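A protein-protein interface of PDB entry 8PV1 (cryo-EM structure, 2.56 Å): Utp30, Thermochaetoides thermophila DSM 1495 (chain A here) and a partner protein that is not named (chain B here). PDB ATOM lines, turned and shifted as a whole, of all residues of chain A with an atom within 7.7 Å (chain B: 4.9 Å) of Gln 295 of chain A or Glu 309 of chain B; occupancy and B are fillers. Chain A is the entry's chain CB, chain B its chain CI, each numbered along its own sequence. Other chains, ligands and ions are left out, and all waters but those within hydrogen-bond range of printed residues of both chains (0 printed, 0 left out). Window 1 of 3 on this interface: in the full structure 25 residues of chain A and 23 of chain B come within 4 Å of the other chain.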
ATOM      1  N   VAL A  18      -6.313 -24.829  -1.235  1.00  0.00           N
ATOM      2  CA  VAL A  18      -7.117 -24.703  -0.027  1.00  0.00           C
ATOM      3  C   VAL A  18      -8.571 -25.041  -0.325  1.00  0.00           C
ATOM      4  O   VAL A  18      -9.261 -24.286  -1.011  1.00  0.00           O
ATOM      5  CB  VAL A  18      -7.005 -23.292   0.574  1.00  0.00           C
ATOM      6  CG1 VAL A  18      -7.685 -23.239   1.934  1.00  0.00           C
ATOM      7  CG2 VAL A  18      -5.549 -22.870   0.679  1.00  0.00           C
ATOM      8  N   VAL A 278       4.470 -20.313   1.049  1.00  0.00           N
ATOM      9  CA  VAL A 278       3.360 -20.608   1.947  1.00  0.00           C
ATOM     10  C   VAL A 278       3.621 -21.897   2.713  1.00  0.00           C
ATOM     11  O   VAL A 278       3.843 -22.958   2.117  1.00  0.00           O
ATOM     12  CB  VAL A 278       2.038 -20.690   1.162  1.00  0.00           C
ATOM     13  CG1 VAL A 278       0.972 -21.392   1.978  1.00  0.00           C
ATOM     14  CG2 VAL A 278       1.574 -19.296   0.772  1.00  0.00           C
ATOM     15  N   ARG A 279       3.620 -21.807   4.043  1.00  0.00           N
ATOM     16  CA  ARG A 279       3.767 -22.985   4.885  1.00  0.00           C
ATOM     17  C   ARG A 279       2.431 -23.415   5.477  1.00  0.00           C
ATOM     18  O   ARG A 279       1.977 -24.536   5.230  1.00  0.00           O
ATOM     19  CB  ARG A 279       4.783 -22.718   5.997  1.00  0.00           C
ATOM     20  CG  ARG A 279       5.169 -23.929   6.824  1.00  0.00           C
ATOM     21  CD  ARG A 279       6.081 -23.511   7.966  1.00  0.00           C
ATOM     22  NE  ARG A 279       6.465 -24.628   8.820  1.00  0.00           N
ATOM     23  CZ  ARG A 279       7.589 -25.319   8.692  1.00  0.00           C
ATOM     24  NH1 ARG A 279       8.474 -25.031   7.752  1.00  0.00           N
ATOM     25  NH2 ARG A 279       7.833 -26.319   9.533  1.00  0.00           N
ATOM     26  N   ASN A 280       1.777 -22.534   6.234  1.00  0.00           N
ATOM     27  CA  ASN A 280       0.598 -22.913   7.002  1.00  0.00           C
ATOM     28  C   ASN A 280      -0.415 -21.777   7.048  1.00  0.00           C
ATOM     29  O   ASN A 280      -0.066 -20.595   7.084  1.00  0.00           O
ATOM     30  CB  ASN A 280       0.977 -23.318   8.433  1.00  0.00           C
ATOM     31  CG  ASN A 280       1.730 -24.631   8.496  1.00  0.00           C
ATOM     32  OD1 ASN A 280       1.390 -25.589   7.803  1.00  0.00           O
ATOM     33  ND2 ASN A 280       2.765 -24.680   9.325  1.00  0.00           N
ATOM     34  N   PHE A 281      -1.694 -22.152   7.056  1.00  0.00           N
ATOM     35  CA  PHE A 281      -2.788 -21.208   7.260  1.00  0.00           C
ATOM     36  C   PHE A 281      -3.581 -21.666   8.474  1.00  0.00           C
ATOM     37  O   PHE A 281      -3.981 -22.831   8.544  1.00  0.00           O
ATOM     38  CB  PHE A 281      -3.716 -21.116   6.042  1.00  0.00           C
ATOM     39  CG  PHE A 281      -3.228 -20.203   4.949  1.00  0.00           C
ATOM     40  CD1 PHE A 281      -1.922 -20.252   4.500  1.00  0.00           C
ATOM     41  CD2 PHE A 281      -4.080 -19.269   4.386  1.00  0.00           C
ATOM     42  CE1 PHE A 281      -1.488 -19.414   3.499  1.00  0.00           C
ATOM     43  CE2 PHE A 281      -3.638 -18.420   3.390  1.00  0.00           C
ATOM     44  CZ  PHE A 281      -2.343 -18.495   2.948  1.00  0.00           C
ATOM     45  N   TYR A 282      -3.826 -20.758   9.414  1.00  0.00           N
ATOM     46  CA  TYR A 282      -4.610 -21.071  10.600  1.00  0.00           C
ATOM     47  C   TYR A 282      -5.745 -20.071  10.754  1.00  0.00           C
ATOM     48  O   TYR A 282      -5.686 -18.952  10.250  1.00  0.00           O
ATOM     49  CB  TYR A 282      -3.767 -21.056  11.881  1.00  0.00           C
ATOM     50  CG  TYR A 282      -2.509 -21.879  11.818  1.00  0.00           C
ATOM     51  CD1 TYR A 282      -2.544 -23.251  12.022  1.00  0.00           C
ATOM     52  CD2 TYR A 282      -1.282 -21.280  11.581  1.00  0.00           C
ATOM     53  CE1 TYR A 282      -1.394 -24.006  11.975  1.00  0.00           C
ATOM     54  CE2 TYR A 282      -0.125 -22.026  11.534  1.00  0.00           C
ATOM     55  CZ  TYR A 282      -0.185 -23.389  11.732  1.00  0.00           C
ATOM     56  OH  TYR A 282       0.969 -24.134  11.683  1.00  0.00           O
ATOM     57  N   LEU A 291      -6.769 -23.389  14.322  1.00  0.00           N
ATOM     58  CA  LEU A 291      -7.286 -24.469  13.499  1.00  0.00           C
ATOM     59  C   LEU A 291      -6.606 -24.395  12.145  1.00  0.00           C
ATOM     60  O   LEU A 291      -6.801 -23.404  11.423  1.00  0.00           O
ATOM     61  CB  LEU A 291      -8.801 -24.358  13.339  1.00  0.00           C
ATOM     62  CG  LEU A 291      -9.649 -23.912  14.531  1.00  0.00           C
ATOM     63  CD1 LEU A 291     -11.121 -23.924  14.160  1.00  0.00           C
ATOM     64  CD2 LEU A 291      -9.406 -24.797  15.738  1.00  0.00           C
ATOM     65  N   PRO A 292      -5.783 -25.371  11.771  1.00  0.00           N
ATOM     66  CA  PRO A 292      -5.149 -25.330  10.448  1.00  0.00           C
ATOM     67  C   PRO A 292      -6.157 -25.603   9.344  1.00  0.00           C
ATOM     68  O   PRO A 292      -6.904 -26.582   9.383  1.00  0.00           O
ATOM     69  CB  PRO A 292      -4.084 -26.431  10.530  1.00  0.00           C
ATOM     70  CG  PRO A 292      -4.538 -27.323  11.632  1.00  0.00           C
ATOM     71  CD  PRO A 292      -5.225 -26.436  12.619  1.00  0.00           C
ATOM     72  N   ILE A 293      -6.174 -24.714   8.355  1.00  0.00           N
ATOM     73  CA  ILE A 293      -6.997 -24.887   7.164  1.00  0.00           C
ATOM     74  C   ILE A 293      -6.174 -25.180   5.923  1.00  0.00           C
ATOM     75  O   ILE A 293      -6.753 -25.511   4.878  1.00  0.00           O
ATOM     76  CB  ILE A 293      -7.897 -23.657   6.922  1.00  0.00           C
ATOM     77  CG1 ILE A 293      -7.044 -22.448   6.540  1.00  0.00           C
ATOM     78  CG2 ILE A 293      -8.748 -23.374   8.145  1.00  0.00           C
ATOM     79  CD1 ILE A 293      -7.833 -21.211   6.182  1.00  0.00           C
ATOM     80  N   TYR A 294      -4.850 -25.062   5.998  1.00  0.00           N
ATOM     81  CA  TYR A 294      -3.959 -25.441   4.910  1.00  0.00           C
ATOM     82  C   TYR A 294      -2.584 -25.722   5.490  1.00  0.00           C
ATOM     83  O   TYR A 294      -2.011 -24.867   6.171  1.00  0.00           O
ATOM     84  CB  TYR A 294      -3.867 -24.348   3.842  1.00  0.00           C
ATOM     85  CG  TYR A 294      -2.976 -24.724   2.681  1.00  0.00           C
ATOM     86  CD1 TYR A 294      -3.406 -25.619   1.709  1.00  0.00           C
ATOM     87  CD2 TYR A 294      -1.700 -24.189   2.562  1.00  0.00           C
ATOM     88  CE1 TYR A 294      -2.588 -25.966   0.648  1.00  0.00           C
ATOM     89  CE2 TYR A 294      -0.877 -24.530   1.507  1.00  0.00           C
ATOM     90  CZ  TYR A 294      -1.325 -25.418   0.553  1.00  0.00           C
ATOM     91  OH  TYR A 294      -0.507 -25.758  -0.499  1.00  0.00           O
ATOM     92  N   GLN A 295      -2.067 -26.917   5.228  1.00  0.00           N
ATOM     93  CA  GLN A 295      -0.724 -27.295   5.632  1.00  0.00           C
ATOM     94  C   GLN A 295       0.010 -27.847   4.419  1.00  0.00           C
ATOM     95  O   GLN A 295      -0.542 -28.635   3.646  1.00  0.00           O
ATOM     96  CB  GLN A 295      -0.756 -28.317   6.775  1.00  0.00           C
ATOM     97  CG  GLN A 295      -1.150 -27.703   8.114  1.00  0.00           C
ATOM     98  CD  GLN A 295      -0.567 -28.441   9.301  1.00  0.00           C
ATOM     99  OE1 GLN A 295      -0.954 -29.571   9.597  1.00  0.00           O
ATOM    100  NE2 GLN A 295       0.371 -27.803   9.989  1.00  0.00           N
ATOM    101  N   THR A 296       1.255 -27.415   4.250  1.00  0.00           N
ATOM    102  CA  THR A 296       2.006 -27.686   3.033  1.00  0.00           C
ATOM    103  C   THR A 296       2.598 -29.095   3.070  1.00  0.00           C
ATOM    104  O   THR A 296       2.539 -29.797   4.082  1.00  0.00           O
ATOM    105  CB  THR A 296       3.090 -26.628   2.843  1.00  0.00           C
ATOM    106  OG1 THR A 296       3.714 -26.802   1.565  1.00  0.00           O
ATOM    107  CG2 THR A 296       4.138 -26.744   3.938  1.00  0.00           C
ATOM    108  N   ASP A 297       3.183 -29.516   1.955  1.00  0.00           N
ATOM    109  CA  ASP A 297       3.859 -30.805   1.847  1.00  0.00           C
ATOM    110  C   ASP A 297       5.371 -30.671   1.743  1.00  0.00           C
ATOM    111  O   ASP A 297       6.091 -31.593   2.133  1.00  0.00           O
ATOM    112  CB  ASP A 297       3.298 -31.603   0.644  1.00  0.00           C
ATOM    113  CG  ASP A 297       3.417 -30.857  -0.680  1.00  0.00           C
ATOM    114  OD1 ASP A 297       3.850 -29.686  -0.689  1.00  0.00           O
ATOM    115  OD2 ASP A 297       3.071 -31.454  -1.723  1.00  0.00           O
ATOM    116  N   GLU A 298       5.869 -29.555   1.215  1.00  0.00           N
ATOM    117  CA  GLU A 298       7.300 -29.278   1.192  1.00  0.00           C
ATOM    118  C   GLU A 298       7.615 -28.154   2.173  1.00  0.00           C
ATOM    119  O   GLU A 298       6.905 -27.144   2.211  1.00  0.00           O
ATOM    120  CB  GLU A 298       7.746 -28.900  -0.217  1.00  0.00           C
ATOM    121  CG  GLU A 298       7.576 -30.009  -1.237  1.00  0.00           C
ATOM    122  CD  GLU A 298       8.017 -29.592  -2.623  1.00  0.00           C
ATOM    123  OE1 GLU A 298       8.371 -28.408  -2.804  1.00  0.00           O
ATOM    124  OE2 GLU A 298       8.009 -30.447  -3.533  1.00  0.00           O
ATOM    125  N   LEU A 299       8.670 -28.327   2.968  1.00  0.00           N
ATOM    126  CA  LEU A 299       9.100 -27.312   3.921  1.00  0.00           C
ATOM    127  C   LEU A 299      10.204 -26.414   3.376  1.00  0.00           C
ATOM    128  O   LEU A 299      10.716 -25.565   4.111  1.00  0.00           O
ATOM    129  CB  LEU A 299       9.559 -27.969   5.224  1.00  0.00           C
ATOM    130  CG  LEU A 299       8.546 -28.892   5.899  1.00  0.00           C
ATOM    131  CD1 LEU A 299       9.182 -29.612   7.076  1.00  0.00           C
ATOM    132  CD2 LEU A 299       7.321 -28.107   6.343  1.00  0.00           C
ATOM    133  N   LYS B 305      14.326 -31.711  11.100  1.00  0.00           N
ATOM    134  CA  LYS B 305      13.297 -30.674  11.065  1.00  0.00           C
ATOM    135  C   LYS B 305      11.935 -31.234  10.685  1.00  0.00           C
ATOM    136  O   LYS B 305      10.925 -30.930  11.341  1.00  0.00           O
ATOM    137  CB  LYS B 305      13.688 -29.581  10.075  1.00  0.00           C
ATOM    138  CG  LYS B 305      14.830 -28.703  10.508  1.00  0.00           C
ATOM    139  CD  LYS B 305      15.068 -27.644   9.452  1.00  0.00           C
ATOM    140  CE  LYS B 305      13.933 -26.630   9.426  1.00  0.00           C
ATOM    141  NZ  LYS B 305      14.197 -25.525   8.459  1.00  0.00           N
ATOM    142  N   VAL B 306      11.884 -32.060   9.632  1.00  0.00           N
ATOM    143  CA  VAL B 306      10.590 -32.543   9.161  1.00  0.00           C
ATOM    144  C   VAL B 306       9.964 -33.453  10.208  1.00  0.00           C
ATOM    145  O   VAL B 306       8.805 -33.248  10.585  1.00  0.00           O
ATOM    146  CB  VAL B 306      10.702 -33.194   7.761  1.00  0.00           C
ATOM    147  CG1 VAL B 306      11.535 -34.481   7.723  1.00  0.00           C
ATOM    148  CG2 VAL B 306       9.312 -33.455   7.178  1.00  0.00           C
ATOM    149  N   ALA B 307      10.773 -34.352  10.805  1.00  0.00           N
ATOM    150  CA  ALA B 307      10.269 -35.292  11.802  1.00  0.00           C
ATOM    151  C   ALA B 307       9.714 -34.554  13.008  1.00  0.00           C
ATOM    152  O   ALA B 307       8.584 -34.828  13.452  1.00  0.00           O
ATOM    153  CB  ALA B 307      11.382 -36.253  12.218  1.00  0.00           C
ATOM    154  N   LYS B 308      10.475 -33.551  13.483  1.00  0.00           N
ATOM    155  CA  LYS B 308      10.021 -32.666  14.549  1.00  0.00           C
ATOM    156  C   LYS B 308       8.673 -32.048  14.221  1.00  0.00           C
ATOM    157  O   LYS B 308       7.776 -32.008  15.076  1.00  0.00           O
ATOM    158  CB  LYS B 308      11.064 -31.575  14.786  1.00  0.00           C
ATOM    159  CG  LYS B 308      10.872 -30.734  16.033  1.00  0.00           C
ATOM    160  CD  LYS B 308      10.279 -29.367  15.672  1.00  0.00           C
ATOM    161  CE  LYS B 308      10.172 -28.447  16.879  1.00  0.00           C
ATOM    162  NZ  LYS B 308       9.544 -27.162  16.472  1.00  0.00           N
ATOM    163  N   GLU B 309       8.482 -31.625  12.972  1.00  0.00           N
ATOM    164  CA  GLU B 309       7.230 -30.945  12.669  1.00  0.00           C
ATOM    165  C   GLU B 309       6.080 -31.946  12.493  1.00  0.00           C
ATOM    166  O   GLU B 309       4.915 -31.568  12.656  1.00  0.00           O
ATOM    167  CB  GLU B 309       7.407 -30.025  11.458  1.00  0.00           C
ATOM    168  CG  GLU B 309       6.261 -29.014  11.153  1.00  0.00           C
ATOM    169  CD  GLU B 309       5.091 -29.511  10.353  1.00  0.00           C
ATOM    170  OE1 GLU B 309       5.266 -30.425   9.544  1.00  0.00           O
ATOM    171  OE2 GLU B 309       3.993 -28.933  10.479  1.00  0.00           O
ATOM    172  N   GLU B 310       6.361 -33.230  12.182  1.00  0.00           N
ATOM    173  CA  GLU B 310       5.245 -34.184  12.297  1.00  0.00           C
ATOM    174  C   GLU B 310       4.820 -34.416  13.746  1.00  0.00           C
ATOM    175  O   GLU B 310       3.624 -34.604  13.993  1.00  0.00           O
ATOM    176  CB  GLU B 310       5.358 -35.574  11.617  1.00  0.00           C
ATOM    177  CG  GLU B 310       5.366 -35.784  10.063  1.00  0.00           C
ATOM    178  CD  GLU B 310       6.659 -35.668   9.334  1.00  0.00           C
ATOM    179  OE1 GLU B 310       7.666 -35.494   9.995  1.00  0.00           O
ATOM    180  OE2 GLU B 310       6.671 -35.832   8.092  1.00  0.00           O
ATOM    181  N   GLN B 311       5.741 -34.447  14.731  1.00  0.00           N
ATOM    182  CA  GLN B 311       5.144 -34.572  16.077  1.00  0.00           C
ATOM    183  C   GLN B 311       4.514 -33.254  16.521  1.00  0.00           C
ATOM    184  O   GLN B 311       3.618 -33.247  17.372  1.00  0.00           O
ATOM    185  CB  GLN B 311       6.019 -35.115  17.236  1.00  0.00           C
ATOM    186  CG  GLN B 311       7.182 -34.329  17.842  1.00  0.00           C
ATOM    187  CD  GLN B 311       8.460 -34.538  17.137  1.00  0.00           C
ATOM    188  OE1 GLN B 311       8.470 -35.034  16.040  1.00  0.00           O
ATOM    189  NE2 GLN B 311       9.566 -34.166  17.769  1.00  0.00           N
ATOM    190  N   ARG B 312       4.936 -32.129  15.936  1.00  0.00           N
ATOM    191  CA  ARG B 312       4.222 -30.877  16.192  1.00  0.00           C
ATOM    192  C   ARG B 312       2.798 -30.930  15.638  1.00  0.00           C
ATOM    193  O   ARG B 312       1.836 -30.535  16.314  1.00  0.00           O
ATOM    194  CB  ARG B 312       4.994 -29.695  15.608  1.00  0.00           C
ATOM    195  CG  ARG B 312       4.241 -28.380  15.714  1.00  0.00           C
ATOM    196  CD  ARG B 312       5.160 -27.189  15.543  1.00  0.00           C
ATOM    197  NE  ARG B 312       5.943 -27.246  14.316  1.00  0.00           N
ATOM    198  CZ  ARG B 312       6.841 -26.337  13.966  1.00  0.00           C
ATOM    199  NH1 ARG B 312       7.088 -25.282  14.727  1.00  0.00           N
ATOM    200  NH2 ARG B 312       7.510 -26.487  12.828  1.00  0.00           N
ATOM    201  N   ARG B 313       2.648 -31.456  14.417  1.00  0.00           N
ATOM    202  CA  ARG B 313       1.322 -31.676  13.844  1.00  0.00           C
ATOM    203  C   ARG B 313       0.515 -32.665  14.670  1.00  0.00           C
ATOM    204  O   ARG B 313      -0.699 -32.505  14.822  1.00  0.00           O
ATOM    205  CB  ARG B 313       1.436 -32.181  12.406  1.00  0.00           C
ATOM    206  CG  ARG B 313       1.740 -31.122  11.375  1.00  0.00           C
ATOM    207  CD  ARG B 313       2.266 -31.754  10.104  1.00  0.00           C
ATOM    208  NE  ARG B 313       2.530 -30.757   9.075  1.00  0.00           N
ATOM    209  CZ  ARG B 313       2.065 -30.826   7.836  1.00  0.00           C
ATOM    210  NH1 ARG B 313       1.374 -31.874   7.416  1.00  0.00           N
ATOM    211  NH2 ARG B 313       2.306 -29.823   6.997  1.00  0.00           N
ATOM    212  N   ARG B 316      -0.718 -30.937  17.796  1.00  0.00           N
ATOM    213  CA  ARG B 316      -1.813 -30.047  17.422  1.00  0.00           C
ATOM    214  C   ARG B 316      -3.089 -30.832  17.126  1.00  0.00           C
ATOM    215  O   ARG B 316      -4.185 -30.416  17.510  1.00  0.00           O
ATOM    216  CB  ARG B 316      -1.402 -29.183  16.229  1.00  0.00           C
ATOM    217  CG  ARG B 316      -0.617 -27.949  16.644  1.00  0.00           C
ATOM    218  CD  ARG B 316      -0.201 -27.100  15.457  1.00  0.00           C
ATOM    219  NE  ARG B 316       0.875 -27.723  14.698  1.00  0.00           N
ATOM    220  CZ  ARG B 316       1.341 -27.263  13.546  1.00  0.00           C
ATOM    221  NH1 ARG B 316       0.852 -26.167  12.993  1.00  0.00           N
ATOM    222  NH2 ARG B 316       2.326 -27.915  12.935  1.00  0.00           N
ATOM    223  N   PHE B 327      -8.736 -32.365  10.782  1.00  0.00           N
ATOM    224  CA  PHE B 327      -7.939 -31.918   9.646  1.00  0.00           C
ATOM    225  C   PHE B 327      -7.069 -33.079   9.192  1.00  0.00           C
ATOM    226  O   PHE B 327      -6.295 -33.624   9.986  1.00  0.00           O
ATOM    227  CB  PHE B 327      -7.069 -30.716  10.015  1.00  0.00           C
ATOM    228  CG  PHE B 327      -6.272 -30.167   8.867  1.00  0.00           C
ATOM    229  CD1 PHE B 327      -4.888 -30.192   8.891  1.00  0.00           C
ATOM    230  CD2 PHE B 327      -6.911 -29.607   7.772  1.00  0.00           C
ATOM    231  CE1 PHE B 327      -4.155 -29.684   7.836  1.00  0.00           C
ATOM    232  CE2 PHE B 327      -6.183 -29.095   6.715  1.00  0.00           C
ATOM    233  CZ  PHE B 327      -4.802 -29.133   6.748  1.00  0.00           C
ATOM    234  N   ALA B 329      -4.011 -33.929   7.629  1.00  0.00           N
ATOM    235  CA  ALA B 329      -2.754 -33.304   7.234  1.00  0.00           C
ATOM    236  C   ALA B 329      -2.058 -34.158   6.183  1.00  0.00           C
ATOM    237  O   ALA B 329      -1.829 -35.351   6.420  1.00  0.00           O
ATOM    238  CB  ALA B 329      -1.840 -33.118   8.437  1.00  0.00           C
ATOM    239  N   PRO B 330      -1.735 -33.598   5.016  1.00  0.00           N
ATOM    240  CA  PRO B 330      -1.064 -34.389   3.975  1.00  0.00           C
ATOM    241  C   PRO B 330       0.331 -34.823   4.399  1.00  0.00           C
ATOM    242  O   PRO B 330       1.015 -34.138   5.161  1.00  0.00           O
ATOM    243  CB  PRO B 330      -1.015 -33.432   2.778  1.00  0.00           C
ATOM    244  CG  PRO B 330      -2.087 -32.429   3.047  1.00  0.00           C
ATOM    245  CD  PRO B 330      -2.111 -32.260   4.532  1.00  0.00           C
ATOM    246  N   LEU B 332       4.152 -35.425   4.462  1.00  0.00           N
ATOM    247  CA  LEU B 332       5.307 -34.688   3.974  1.00  0.00           C
ATOM    248  C   LEU B 332       6.218 -35.610   3.173  1.00  0.00           C
ATOM    249  O   LEU B 332       6.642 -36.659   3.669  1.00  0.00           O
ATOM    250  CB  LEU B 332       6.056 -34.067   5.155  1.00  0.00           C
ATOM    251  CG  LEU B 332       5.134 -33.188   6.012  1.00  0.00           C
ATOM    252  CD1 LEU B 332       5.645 -32.935   7.416  1.00  0.00           C
ATOM    253  CD2 LEU B 332       4.893 -31.871   5.318  1.00  0.00           C
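The guanidinium group (NH1) of Arg 316 of chain B lies within hydrogen-bond range of the side-chain hydroxyl (OH) of Tyr 282 of chain A (2.4 Å). The guanidinium group (NH1) of Arg 316 of chain B lies close to the side-chain amide nitrogen (NE2) of Gln 295 of chain A (3.5 Å). The backbone carbonyl oxygen of Thr 296 of chain A lies within hydrogen-bond range of the guanidinium group of Arg 313 of chain B (2.9 Å). NH2 of Arg 279 of chain A lies close to NH2 of Arg 312 of chain B, at 3.3 Å.
N of Thr 296 of chain A sits at hydrogen-bond distance from O of Arg 279 of chain A (3.1 Å). ND2 of Asn 280 of chain A lies within hydrogen-bond range of OH of Tyr 282 of chain A (3.0 Å). O of Phe 281 of chain A sits at hydrogen-bond distance from N of Ile 293 of chain A, 2.9 Å away. O of Val 306 of chain B sits close to OE1 of Glu 310 of chain B (2.6 Å). NH2 of Arg 316 of chain B lies within salt-bridge range of OE2 of Glu 309 of chain B. NH1 of Arg 313 of chain B lies within hydrogen-bond range of O of Pro 330 of chain B, at 3.2 Å.
Tyr 294 of chain A touches none of the printed residues of chain B. Printed residues of chain B within 4 Å of Gln 295 of chain A: Glu 309, Arg 313, Arg 316, Phe 327 and Ala 329. Printed residues of chain A within 4 Å of Arg 313 of chain B: Gln 295 (3.4 Å) and Thr 296 (2.9 Å). Of the printed residues of chain A, Arg 316 of chain B touches Tyr 282 (2.4 Å) and Gln 295 (3.5 Å). The nearest residue of chain B that does not touch Gln 295 of chain A is Pro 330 of chain B (4.05 Å). The nearest printed residue of chain B that does not touch Asp 297 of chain A is Arg 313 of chain B (5.1 Å).
Printed residues of chain B that touch a printed residue of chain A: Val 306, Glu 309, Arg 312, Arg 313, Arg 316, Phe 327, Ala 329 and Leu 332. Hydrophobic or aromatic side chains of chain B that line the printed part of chain A: Val 306, Phe 327, Ala 329 and Leu 332.
Among the printed residues, merely in contact across the chains: Arg 279 of chain A with Glu 309 of chain B, Pro 292 of chain A with Phe 327 of chain B, Ile 293 of chain A with Phe 327 of chain B, Gln 295 of chain A with Glu 309 of chain B, Gln 295 of chain A with Arg 313 of chain B, Gln 295 of chain A with Phe 327 of chain B, Gln 295 of chain A with Ala 329 of chain B, Thr 296 of chain A with Leu 332 of chain B, Asp 297 of chain A with Leu 332 of chain B and Leu 299 of chain A with Val 306 of chain B.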
